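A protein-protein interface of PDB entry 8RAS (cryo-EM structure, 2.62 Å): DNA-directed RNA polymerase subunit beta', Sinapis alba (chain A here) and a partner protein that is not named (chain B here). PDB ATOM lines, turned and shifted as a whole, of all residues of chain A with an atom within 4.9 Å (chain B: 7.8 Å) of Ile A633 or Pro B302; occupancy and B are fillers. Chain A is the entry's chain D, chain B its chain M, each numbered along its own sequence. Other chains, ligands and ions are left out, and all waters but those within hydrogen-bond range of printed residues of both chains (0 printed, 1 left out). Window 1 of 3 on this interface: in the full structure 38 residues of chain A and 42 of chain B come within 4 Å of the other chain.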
ATOM      1  N   TRP A 603      30.496 -17.883  21.576  1.00  0.00           N
ATOM      2  CA  TRP A 603      29.482 -17.203  22.366  1.00  0.00           C
ATOM      3  C   TRP A 603      29.743 -15.705  22.328  1.00  0.00           C
ATOM      4  O   TRP A 603      30.857 -15.257  22.619  1.00  0.00           O
ATOM      5  CB  TRP A 603      29.479 -17.708  23.808  1.00  0.00           C
ATOM      6  CG  TRP A 603      28.958 -19.101  23.949  1.00  0.00           C
ATOM      7  CD1 TRP A 603      29.691 -20.249  23.976  1.00  0.00           C
ATOM      8  CD2 TRP A 603      27.588 -19.496  24.082  1.00  0.00           C
ATOM      9  NE1 TRP A 603      28.863 -21.335  24.117  1.00  0.00           N
ATOM     10  CE2 TRP A 603      27.568 -20.899  24.185  1.00  0.00           C
ATOM     11  CE3 TRP A 603      26.378 -18.797  24.124  1.00  0.00           C
ATOM     12  CZ2 TRP A 603      26.384 -21.617  24.329  1.00  0.00           C
ATOM     13  CZ3 TRP A 603      25.206 -19.513  24.266  1.00  0.00           C
ATOM     14  CH2 TRP A 603      25.218 -20.907  24.367  1.00  0.00           C
ATOM     15  N   PRO A 619      13.430 -23.249  27.038  1.00  0.00           N
ATOM     16  CA  PRO A 619      14.835 -23.629  27.232  1.00  0.00           C
ATOM     17  C   PRO A 619      15.007 -25.138  27.278  1.00  0.00           C
ATOM     18  O   PRO A 619      14.156 -25.866  27.794  1.00  0.00           O
ATOM     19  CB  PRO A 619      15.197 -22.989  28.577  1.00  0.00           C
ATOM     20  CG  PRO A 619      14.180 -21.947  28.808  1.00  0.00           C
ATOM     21  CD  PRO A 619      12.932 -22.403  28.136  1.00  0.00           C
ATOM     22  N   ILE A 620      16.123 -25.607  26.719  1.00  0.00           N
ATOM     23  CA  ILE A 620      16.476 -27.017  26.844  1.00  0.00           C
ATOM     24  C   ILE A 620      16.720 -27.369  28.301  1.00  0.00           C
ATOM     25  O   ILE A 620      16.257 -28.404  28.795  1.00  0.00           O
ATOM     26  CB  ILE A 620      17.710 -27.346  25.986  1.00  0.00           C
ATOM     27  CG1 ILE A 620      17.477 -26.977  24.521  1.00  0.00           C
ATOM     28  CG2 ILE A 620      18.063 -28.809  26.133  1.00  0.00           C
ATOM     29  CD1 ILE A 620      18.757 -26.754  23.751  1.00  0.00           C
ATOM     30  N   GLU A 621      17.451 -26.516  29.010  1.00  0.00           N
ATOM     31  CA  GLU A 621      17.854 -26.794  30.378  1.00  0.00           C
ATOM     32  C   GLU A 621      17.880 -25.490  31.157  1.00  0.00           C
ATOM     33  O   GLU A 621      18.375 -24.475  30.662  1.00  0.00           O
ATOM     34  CB  GLU A 621      19.229 -27.465  30.416  1.00  0.00           C
ATOM     35  CG  GLU A 621      19.467 -28.337  31.626  1.00  0.00           C
ATOM     36  CD  GLU A 621      20.534 -29.384  31.384  1.00  0.00           C
ATOM     37  OE1 GLU A 621      20.383 -30.181  30.434  1.00  0.00           O
ATOM     38  OE2 GLU A 621      21.525 -29.411  32.144  1.00  0.00           O
ATOM     39  N   HIS A 623      19.321 -24.102  34.735  1.00  0.00           N
ATOM     40  CA  HIS A 623      20.225 -24.393  35.844  1.00  0.00           C
ATOM     41  C   HIS A 623      19.949 -23.381  36.949  1.00  0.00           C
ATOM     42  O   HIS A 623      20.473 -22.265  36.930  1.00  0.00           O
ATOM     43  CB  HIS A 623      21.677 -24.349  35.388  1.00  0.00           C
ATOM     44  CG  HIS A 623      22.062 -25.482  34.491  1.00  0.00           C
ATOM     45  ND1 HIS A 623      23.219 -25.479  33.742  1.00  0.00           N
ATOM     46  CD2 HIS A 623      21.442 -26.655  34.222  1.00  0.00           C
ATOM     47  CE1 HIS A 623      23.295 -26.602  33.051  1.00  0.00           C
ATOM     48  NE2 HIS A 623      22.229 -27.332  33.324  1.00  0.00           N
ATOM     49  N   HIS A 631      20.234 -20.035  35.115  1.00  0.00           N
ATOM     50  CA  HIS A 631      20.701 -19.947  33.737  1.00  0.00           C
ATOM     51  C   HIS A 631      19.724 -20.695  32.844  1.00  0.00           C
ATOM     52  O   HIS A 631      19.474 -21.885  33.056  1.00  0.00           O
ATOM     53  CB  HIS A 631      22.106 -20.531  33.592  1.00  0.00           C
ATOM     54  CG  HIS A 631      23.156 -19.785  34.351  1.00  0.00           C
ATOM     55  ND1 HIS A 631      23.147 -19.677  35.725  1.00  0.00           N
ATOM     56  CD2 HIS A 631      24.253 -19.112  33.929  1.00  0.00           C
ATOM     57  CE1 HIS A 631      24.191 -18.968  36.116  1.00  0.00           C
ATOM     58  NE2 HIS A 631      24.878 -18.614  35.045  1.00  0.00           N
ATOM     59  N   GLU A 632      19.182 -20.003  31.849  1.00  0.00           N
ATOM     60  CA  GLU A 632      18.278 -20.604  30.880  1.00  0.00           C
ATOM     61  C   GLU A 632      19.045 -20.853  29.589  1.00  0.00           C
ATOM     62  O   GLU A 632      19.544 -19.910  28.967  1.00  0.00           O
ATOM     63  CB  GLU A 632      17.068 -19.707  30.635  1.00  0.00           C
ATOM     64  CG  GLU A 632      16.115 -19.633  31.813  1.00  0.00           C
ATOM     65  CD  GLU A 632      15.017 -18.612  31.613  1.00  0.00           C
ATOM     66  OE1 GLU A 632      15.328 -17.474  31.205  1.00  0.00           O
ATOM     67  OE2 GLU A 632      13.841 -18.948  31.863  1.00  0.00           O
ATOM     68  N   ILE A 633      19.136 -22.117  29.189  1.00  0.00           N
ATOM     69  CA  ILE A 633      19.922 -22.529  28.034  1.00  0.00           C
ATOM     70  C   ILE A 633      18.955 -22.871  26.910  1.00  0.00           C
ATOM     71  O   ILE A 633      18.196 -23.842  27.004  1.00  0.00           O
ATOM     72  CB  ILE A 633      20.837 -23.715  28.361  1.00  0.00           C
ATOM     73  CG1 ILE A 633      21.866 -23.317  29.419  1.00  0.00           C
ATOM     74  CG2 ILE A 633      21.531 -24.212  27.107  1.00  0.00           C
ATOM     75  CD1 ILE A 633      22.235 -24.436  30.360  1.00  0.00           C
ATOM     76  N   TYR A 634      18.983 -22.077  25.849  1.00  0.00           N
ATOM     77  CA  TYR A 634      18.186 -22.322  24.661  1.00  0.00           C
ATOM     78  C   TYR A 634      19.054 -22.976  23.591  1.00  0.00           C
ATOM     79  O   TYR A 634      20.220 -23.308  23.812  1.00  0.00           O
ATOM     80  CB  TYR A 634      17.562 -21.022  24.150  1.00  0.00           C
ATOM     81  CG  TYR A 634      16.578 -20.392  25.109  1.00  0.00           C
ATOM     82  CD1 TYR A 634      17.015 -19.668  26.208  1.00  0.00           C
ATOM     83  CD2 TYR A 634      15.211 -20.519  24.911  1.00  0.00           C
ATOM     84  CE1 TYR A 634      16.121 -19.095  27.085  1.00  0.00           C
ATOM     85  CE2 TYR A 634      14.310 -19.947  25.781  1.00  0.00           C
ATOM     86  CZ  TYR A 634      14.770 -19.235  26.866  1.00  0.00           C
ATOM     87  OH  TYR A 634      13.876 -18.662  27.739  1.00  0.00           O
ATOM     88  N   ALA A 635      18.470 -23.162  22.407  1.00  0.00           N
ATOM     89  CA  ALA A 635      19.208 -23.788  21.319  1.00  0.00           C
ATOM     90  C   ALA A 635      20.290 -22.872  20.765  1.00  0.00           C
ATOM     91  O   ALA A 635      21.316 -23.356  20.275  1.00  0.00           O
ATOM     92  CB  ALA A 635      18.248 -24.208  20.207  1.00  0.00           C
ATOM     93  N   TYR A 637      20.993 -19.429  22.372  1.00  0.00           N
ATOM     94  CA  TYR A 637      21.452 -18.381  23.272  1.00  0.00           C
ATOM     95  C   TYR A 637      21.319 -18.847  24.712  1.00  0.00           C
ATOM     96  O   TYR A 637      20.606 -19.806  25.014  1.00  0.00           O
ATOM     97  CB  TYR A 637      20.692 -17.064  23.068  1.00  0.00           C
ATOM     98  CG  TYR A 637      19.222 -17.207  22.759  1.00  0.00           C
ATOM     99  CD1 TYR A 637      18.773 -17.290  21.449  1.00  0.00           C
ATOM    100  CD2 TYR A 637      18.280 -17.237  23.776  1.00  0.00           C
ATOM    101  CE1 TYR A 637      17.429 -17.415  21.162  1.00  0.00           C
ATOM    102  CE2 TYR A 637      16.936 -17.359  23.500  1.00  0.00           C
ATOM    103  CZ  TYR A 637      16.515 -17.447  22.192  1.00  0.00           C
ATOM    104  OH  TYR A 637      15.175 -17.570  21.912  1.00  0.00           O
ATOM    105  N   LEU A 638      22.026 -18.148  25.594  1.00  0.00           N
ATOM    106  CA  LEU A 638      21.997 -18.394  27.027  1.00  0.00           C
ATOM    107  C   LEU A 638      21.622 -17.102  27.736  1.00  0.00           C
ATOM    108  O   LEU A 638      22.197 -16.047  27.452  1.00  0.00           O
ATOM    109  CB  LEU A 638      23.352 -18.905  27.525  1.00  0.00           C
ATOM    110  CG  LEU A 638      23.666 -18.699  29.007  1.00  0.00           C
ATOM    111  CD1 LEU A 638      23.023 -19.785  29.850  1.00  0.00           C
ATOM    112  CD2 LEU A 638      25.167 -18.658  29.230  1.00  0.00           C
ATOM    113  N   TYR B 200       8.696 -19.070  32.939  1.00  0.00           N
ATOM    114  CA  TYR B 200       9.218 -20.084  32.035  1.00  0.00           C
ATOM    115  C   TYR B 200       8.490 -19.965  30.707  1.00  0.00           C
ATOM    116  O   TYR B 200       7.257 -19.975  30.673  1.00  0.00           O
ATOM    117  CB  TYR B 200       9.035 -21.485  32.630  1.00  0.00           C
ATOM    118  CG  TYR B 200       9.628 -22.613  31.819  1.00  0.00           C
ATOM    119  CD1 TYR B 200      10.958 -22.978  31.971  1.00  0.00           C
ATOM    120  CD2 TYR B 200       8.853 -23.329  30.919  1.00  0.00           C
ATOM    121  CE1 TYR B 200      11.501 -24.013  31.241  1.00  0.00           C
ATOM    122  CE2 TYR B 200       9.388 -24.363  30.184  1.00  0.00           C
ATOM    123  CZ  TYR B 200      10.711 -24.702  30.349  1.00  0.00           C
ATOM    124  OH  TYR B 200      11.250 -25.735  29.618  1.00  0.00           O
ATOM    125  N   ILE B 284      15.960 -28.128  35.304  1.00  0.00           N
ATOM    126  CA  ILE B 284      14.590 -28.235  34.812  1.00  0.00           C
ATOM    127  C   ILE B 284      14.643 -28.534  33.322  1.00  0.00           C
ATOM    128  O   ILE B 284      15.214 -27.757  32.547  1.00  0.00           O
ATOM    129  CB  ILE B 284      13.780 -26.960  35.087  1.00  0.00           C
ATOM    130  CG1 ILE B 284      14.020 -26.470  36.515  1.00  0.00           C
ATOM    131  CG2 ILE B 284      12.303 -27.209  34.853  1.00  0.00           C
ATOM    132  CD1 ILE B 284      13.475 -25.089  36.785  1.00  0.00           C
ATOM    133  N   ARG B 299      27.922 -29.347  37.417  1.00  0.00           N
ATOM    134  CA  ARG B 299      27.211 -28.484  36.484  1.00  0.00           C
ATOM    135  C   ARG B 299      27.632 -28.791  35.052  1.00  0.00           C
ATOM    136  O   ARG B 299      28.799 -29.086  34.779  1.00  0.00           O
ATOM    137  CB  ARG B 299      27.504 -27.021  36.816  1.00  0.00           C
ATOM    138  CG  ARG B 299      26.608 -26.000  36.142  1.00  0.00           C
ATOM    139  CD  ARG B 299      26.972 -24.601  36.621  1.00  0.00           C
ATOM    140  NE  ARG B 299      25.812 -23.801  36.991  1.00  0.00           N
ATOM    141  CZ  ARG B 299      25.022 -23.177  36.127  1.00  0.00           C
ATOM    142  NH1 ARG B 299      25.225 -23.256  34.823  1.00  0.00           N
ATOM    143  NH2 ARG B 299      24.005 -22.453  36.585  1.00  0.00           N
ATOM    144  N   ASP B 300      26.675 -28.719  34.133  1.00  0.00           N
ATOM    145  CA  ASP B 300      26.923 -28.988  32.724  1.00  0.00           C
ATOM    146  C   ASP B 300      27.052 -27.683  31.952  1.00  0.00           C
ATOM    147  O   ASP B 300      26.279 -26.743  32.160  1.00  0.00           O
ATOM    148  CB  ASP B 300      25.803 -29.840  32.125  1.00  0.00           C
ATOM    149  CG  ASP B 300      26.088 -31.324  32.219  1.00  0.00           C
ATOM    150  OD1 ASP B 300      27.178 -31.749  31.785  1.00  0.00           O
ATOM    151  OD2 ASP B 300      25.221 -32.066  32.726  1.00  0.00           O
ATOM    152  N   ASP B 301      28.039 -27.631  31.062  1.00  0.00           N
ATOM    153  CA  ASP B 301      28.239 -26.460  30.228  1.00  0.00           C
ATOM    154  C   ASP B 301      27.060 -26.282  29.271  1.00  0.00           C
ATOM    155  O   ASP B 301      26.472 -27.264  28.810  1.00  0.00           O
ATOM    156  CB  ASP B 301      29.533 -26.594  29.431  1.00  0.00           C
ATOM    157  CG  ASP B 301      30.415 -25.370  29.538  1.00  0.00           C
ATOM    158  OD1 ASP B 301      30.174 -24.538  30.437  1.00  0.00           O
ATOM    159  OD2 ASP B 301      31.352 -25.243  28.724  1.00  0.00           O
ATOM    160  N   PRO B 302      26.683 -25.034  28.970  1.00  0.00           N
ATOM    161  CA  PRO B 302      25.636 -24.822  27.954  1.00  0.00           C
ATOM    162  C   PRO B 302      26.005 -25.405  26.603  1.00  0.00           C
ATOM    163  O   PRO B 302      25.138 -25.939  25.893  1.00  0.00           O
ATOM    164  CB  PRO B 302      25.505 -23.293  27.900  1.00  0.00           C
ATOM    165  CG  PRO B 302      26.093 -22.803  29.177  1.00  0.00           C
ATOM    166  CD  PRO B 302      27.167 -23.771  29.546  1.00  0.00           C
ATOM    167  N   THR B 303      27.286 -25.321  26.237  1.00  0.00           N
ATOM    168  CA  THR B 303      27.755 -25.953  25.010  1.00  0.00           C
ATOM    169  C   THR B 303      27.497 -27.450  25.040  1.00  0.00           C
ATOM    170  O   THR B 303      27.060 -28.031  24.042  1.00  0.00           O
ATOM    171  CB  THR B 303      29.246 -25.672  24.814  1.00  0.00           C
ATOM    172  OG1 THR B 303      29.451 -24.267  24.636  1.00  0.00           O
ATOM    173  CG2 THR B 303      29.774 -26.413  23.599  1.00  0.00           C
ATOM    174  N   THR B 304      27.751 -28.089  26.184  1.00  0.00           N
ATOM    175  CA  THR B 304      27.522 -29.525  26.298  1.00  0.00           C
ATOM    176  C   THR B 304      26.048 -29.869  26.123  1.00  0.00           C
ATOM    177  O   THR B 304      25.712 -30.851  25.456  1.00  0.00           O
ATOM    178  CB  THR B 304      28.034 -30.030  27.646  1.00  0.00           C
ATOM    179  OG1 THR B 304      29.346 -29.507  27.885  1.00  0.00           O
ATOM    180  CG2 THR B 304      28.098 -31.545  27.655  1.00  0.00           C
ATOM    181  N   VAL B 305      25.153 -29.067  26.706  1.00  0.00           N
ATOM    182  CA  VAL B 305      23.720 -29.335  26.592  1.00  0.00           C
ATOM    183  C   VAL B 305      23.266 -29.202  25.141  1.00  0.00           C
ATOM    184  O   VAL B 305      22.563 -30.073  24.601  1.00  0.00           O
ATOM    185  CB  VAL B 305      22.931 -28.392  27.517  1.00  0.00           C
ATOM    186  CG1 VAL B 305      21.448 -28.684  27.437  1.00  0.00           C
ATOM    187  CG2 VAL B 305      23.426 -28.514  28.947  1.00  0.00           C
ATOM    188  N   ILE B 306      23.667 -28.108  24.489  1.00  0.00           N
ATOM    189  CA  ILE B 306      23.272 -27.890  23.101  1.00  0.00           C
ATOM    190  C   ILE B 306      23.827 -28.994  22.211  1.00  0.00           C
ATOM    191  O   ILE B 306      23.129 -29.517  21.332  1.00  0.00           O
ATOM    192  CB  ILE B 306      23.722 -26.494  22.632  1.00  0.00           C
ATOM    193  CG1 ILE B 306      23.021 -25.410  23.451  1.00  0.00           C
ATOM    194  CG2 ILE B 306      23.441 -26.306  21.151  1.00  0.00           C
ATOM    195  CD1 ILE B 306      23.539 -24.017  23.191  1.00  0.00           C
ATOM    196  N   GLU B 307      25.088 -29.377  22.434  1.00  0.00           N
ATOM    197  CA  GLU B 307      25.706 -30.419  21.627  1.00  0.00           C
ATOM    198  C   GLU B 307      25.046 -31.770  21.860  1.00  0.00           C
ATOM    199  O   GLU B 307      24.908 -32.560  20.924  1.00  0.00           O
ATOM    200  CB  GLU B 307      27.202 -30.489  21.925  1.00  0.00           C
ATOM    201  CG  GLU B 307      28.006 -29.382  21.269  1.00  0.00           C
ATOM    202  CD  GLU B 307      29.497 -29.626  21.337  1.00  0.00           C
ATOM    203  OE1 GLU B 307      29.960 -30.226  22.330  1.00  0.00           O
ATOM    204  OE2 GLU B 307      30.209 -29.215  20.397  1.00  0.00           O
ATOM    205  N   ARG B 308      24.634 -32.056  23.096  1.00  0.00           N
ATOM    206  CA  ARG B 308      23.933 -33.305  23.375  1.00  0.00           C
ATOM    207  C   ARG B 308      22.619 -33.372  22.612  1.00  0.00           C
ATOM    208  O   ARG B 308      22.305 -34.386  21.970  1.00  0.00           O
ATOM    209  CB  ARG B 308      23.687 -33.441  24.876  1.00  0.00           C
ATOM    210  CG  ARG B 308      24.853 -34.007  25.653  1.00  0.00           C
ATOM    211  CD  ARG B 308      24.540 -34.070  27.136  1.00  0.00           C
ATOM    212  NE  ARG B 308      25.737 -34.294  27.938  1.00  0.00           N
ATOM    213  CZ  ARG B 308      25.910 -33.830  29.168  1.00  0.00           C
ATOM    214  NH1 ARG B 308      24.980 -33.110  29.774  1.00  0.00           N
ATOM    215  NH2 ARG B 308      27.045 -34.096  29.807  1.00  0.00           N
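OG1 of Thr B303 sits at hydrogen-bond distance from NE1 of Trp A603, at 3.0 Å.
The guanidinium group (NH1) of Arg B299 sits at hydrogen-bond distance from a ring nitrogen (ND1) of His A623 (3.2 Å).
NH2 of Arg B299 lies within hydrogen-bond range of ND1 of His A631 (3.0 Å).
The side-chain hydroxyl of Tyr B200 is in hydrogen-bond range of the backbone carbonyl oxygen of Pro A619, 3.4 Å away.
The side-chain carboxylate (OD1) of Asp B300 lies within salt-bridge range of the guanidinium group (NH2) of Arg B308, 3.1 Å away.
The backbone NH (N) of Ile A620 lies within hydrogen-bond range of the backbone carbonyl oxygen (O) of Ile A633 (2.7 Å).
The side-chain carboxylate of Glu A621 sits at hydrogen-bond distance from a ring nitrogen (NE2) of His A623, at 2.5 Å.
N of His A623 lies within hydrogen-bond range of O of His A631.
The backbone NH (N) of Ile A633 lies within hydrogen-bond range of the backbone carbonyl oxygen (O) of Glu A621 (2.9 Å).
CD1 of Ile B306 touches CH2 of Trp A603, 3.7 Å away.
Ile A620 touches Ile B284.
Val B305 touches Ile A620 (CG1 to CG2, 3.6 Å).
Glu A621 touches Ile B284.
CG1 of Val B305 touches OE1 of Glu A621, at 3.5 Å.
O of Asp B300 touches CE1 of His A623, 3.1 Å away.
CG1 of Ile A633 touches CB of Pro B302, 3.9 Å away.
Ile B306 touches Tyr A634.
Ile B306 touches Ala A635 (CD1 to O, 3.7 Å).
Ile A633 touches just one residue of chain B: Pro B302.
Pro B302 touches just one residue of chain A: Ile A633 (3.9 Å).
Of the printed residues of chain B, Ile A620 touches Ile B284 (3.9 Å) and Val B305 (3.6 Å).
Of the printed residues of chain B, His A623 touches Arg B299 and Asp B300.
Of the printed residues of chain B, Pro A619 touches Tyr B200.
Printed residues of chain A within 4 Å of Asp B300: His A623 (3.1 Å).
Asp B301 touches none of the printed residues of chain A.
Tyr A637 touches none of the printed residues of chain B.
The nearest residue of chain A that does not touch Pro B302 is Trp A603 (4.04 Å).
The nearest printed residue of chain A that does not touch Asp B300 is Glu A621 (4.3 Å).
Of the 12 printed residues of chain B, 8 touch a printed residue of chain A.
Hydrophobic or aromatic side chains of chain B that line the printed part of chain A: Tyr B200, Pro B302, Val B305 and Ile B306.
Along chain B the printed residues that touch a printed residue of chain A span positions 200 to 306.
Among the printed residues, 13 pairs touch across the chains.
Among the printed residues, no Asp or Glu carboxylate lies within 4 Å of a Lys or Arg side-chain nitrogen of the other chain.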
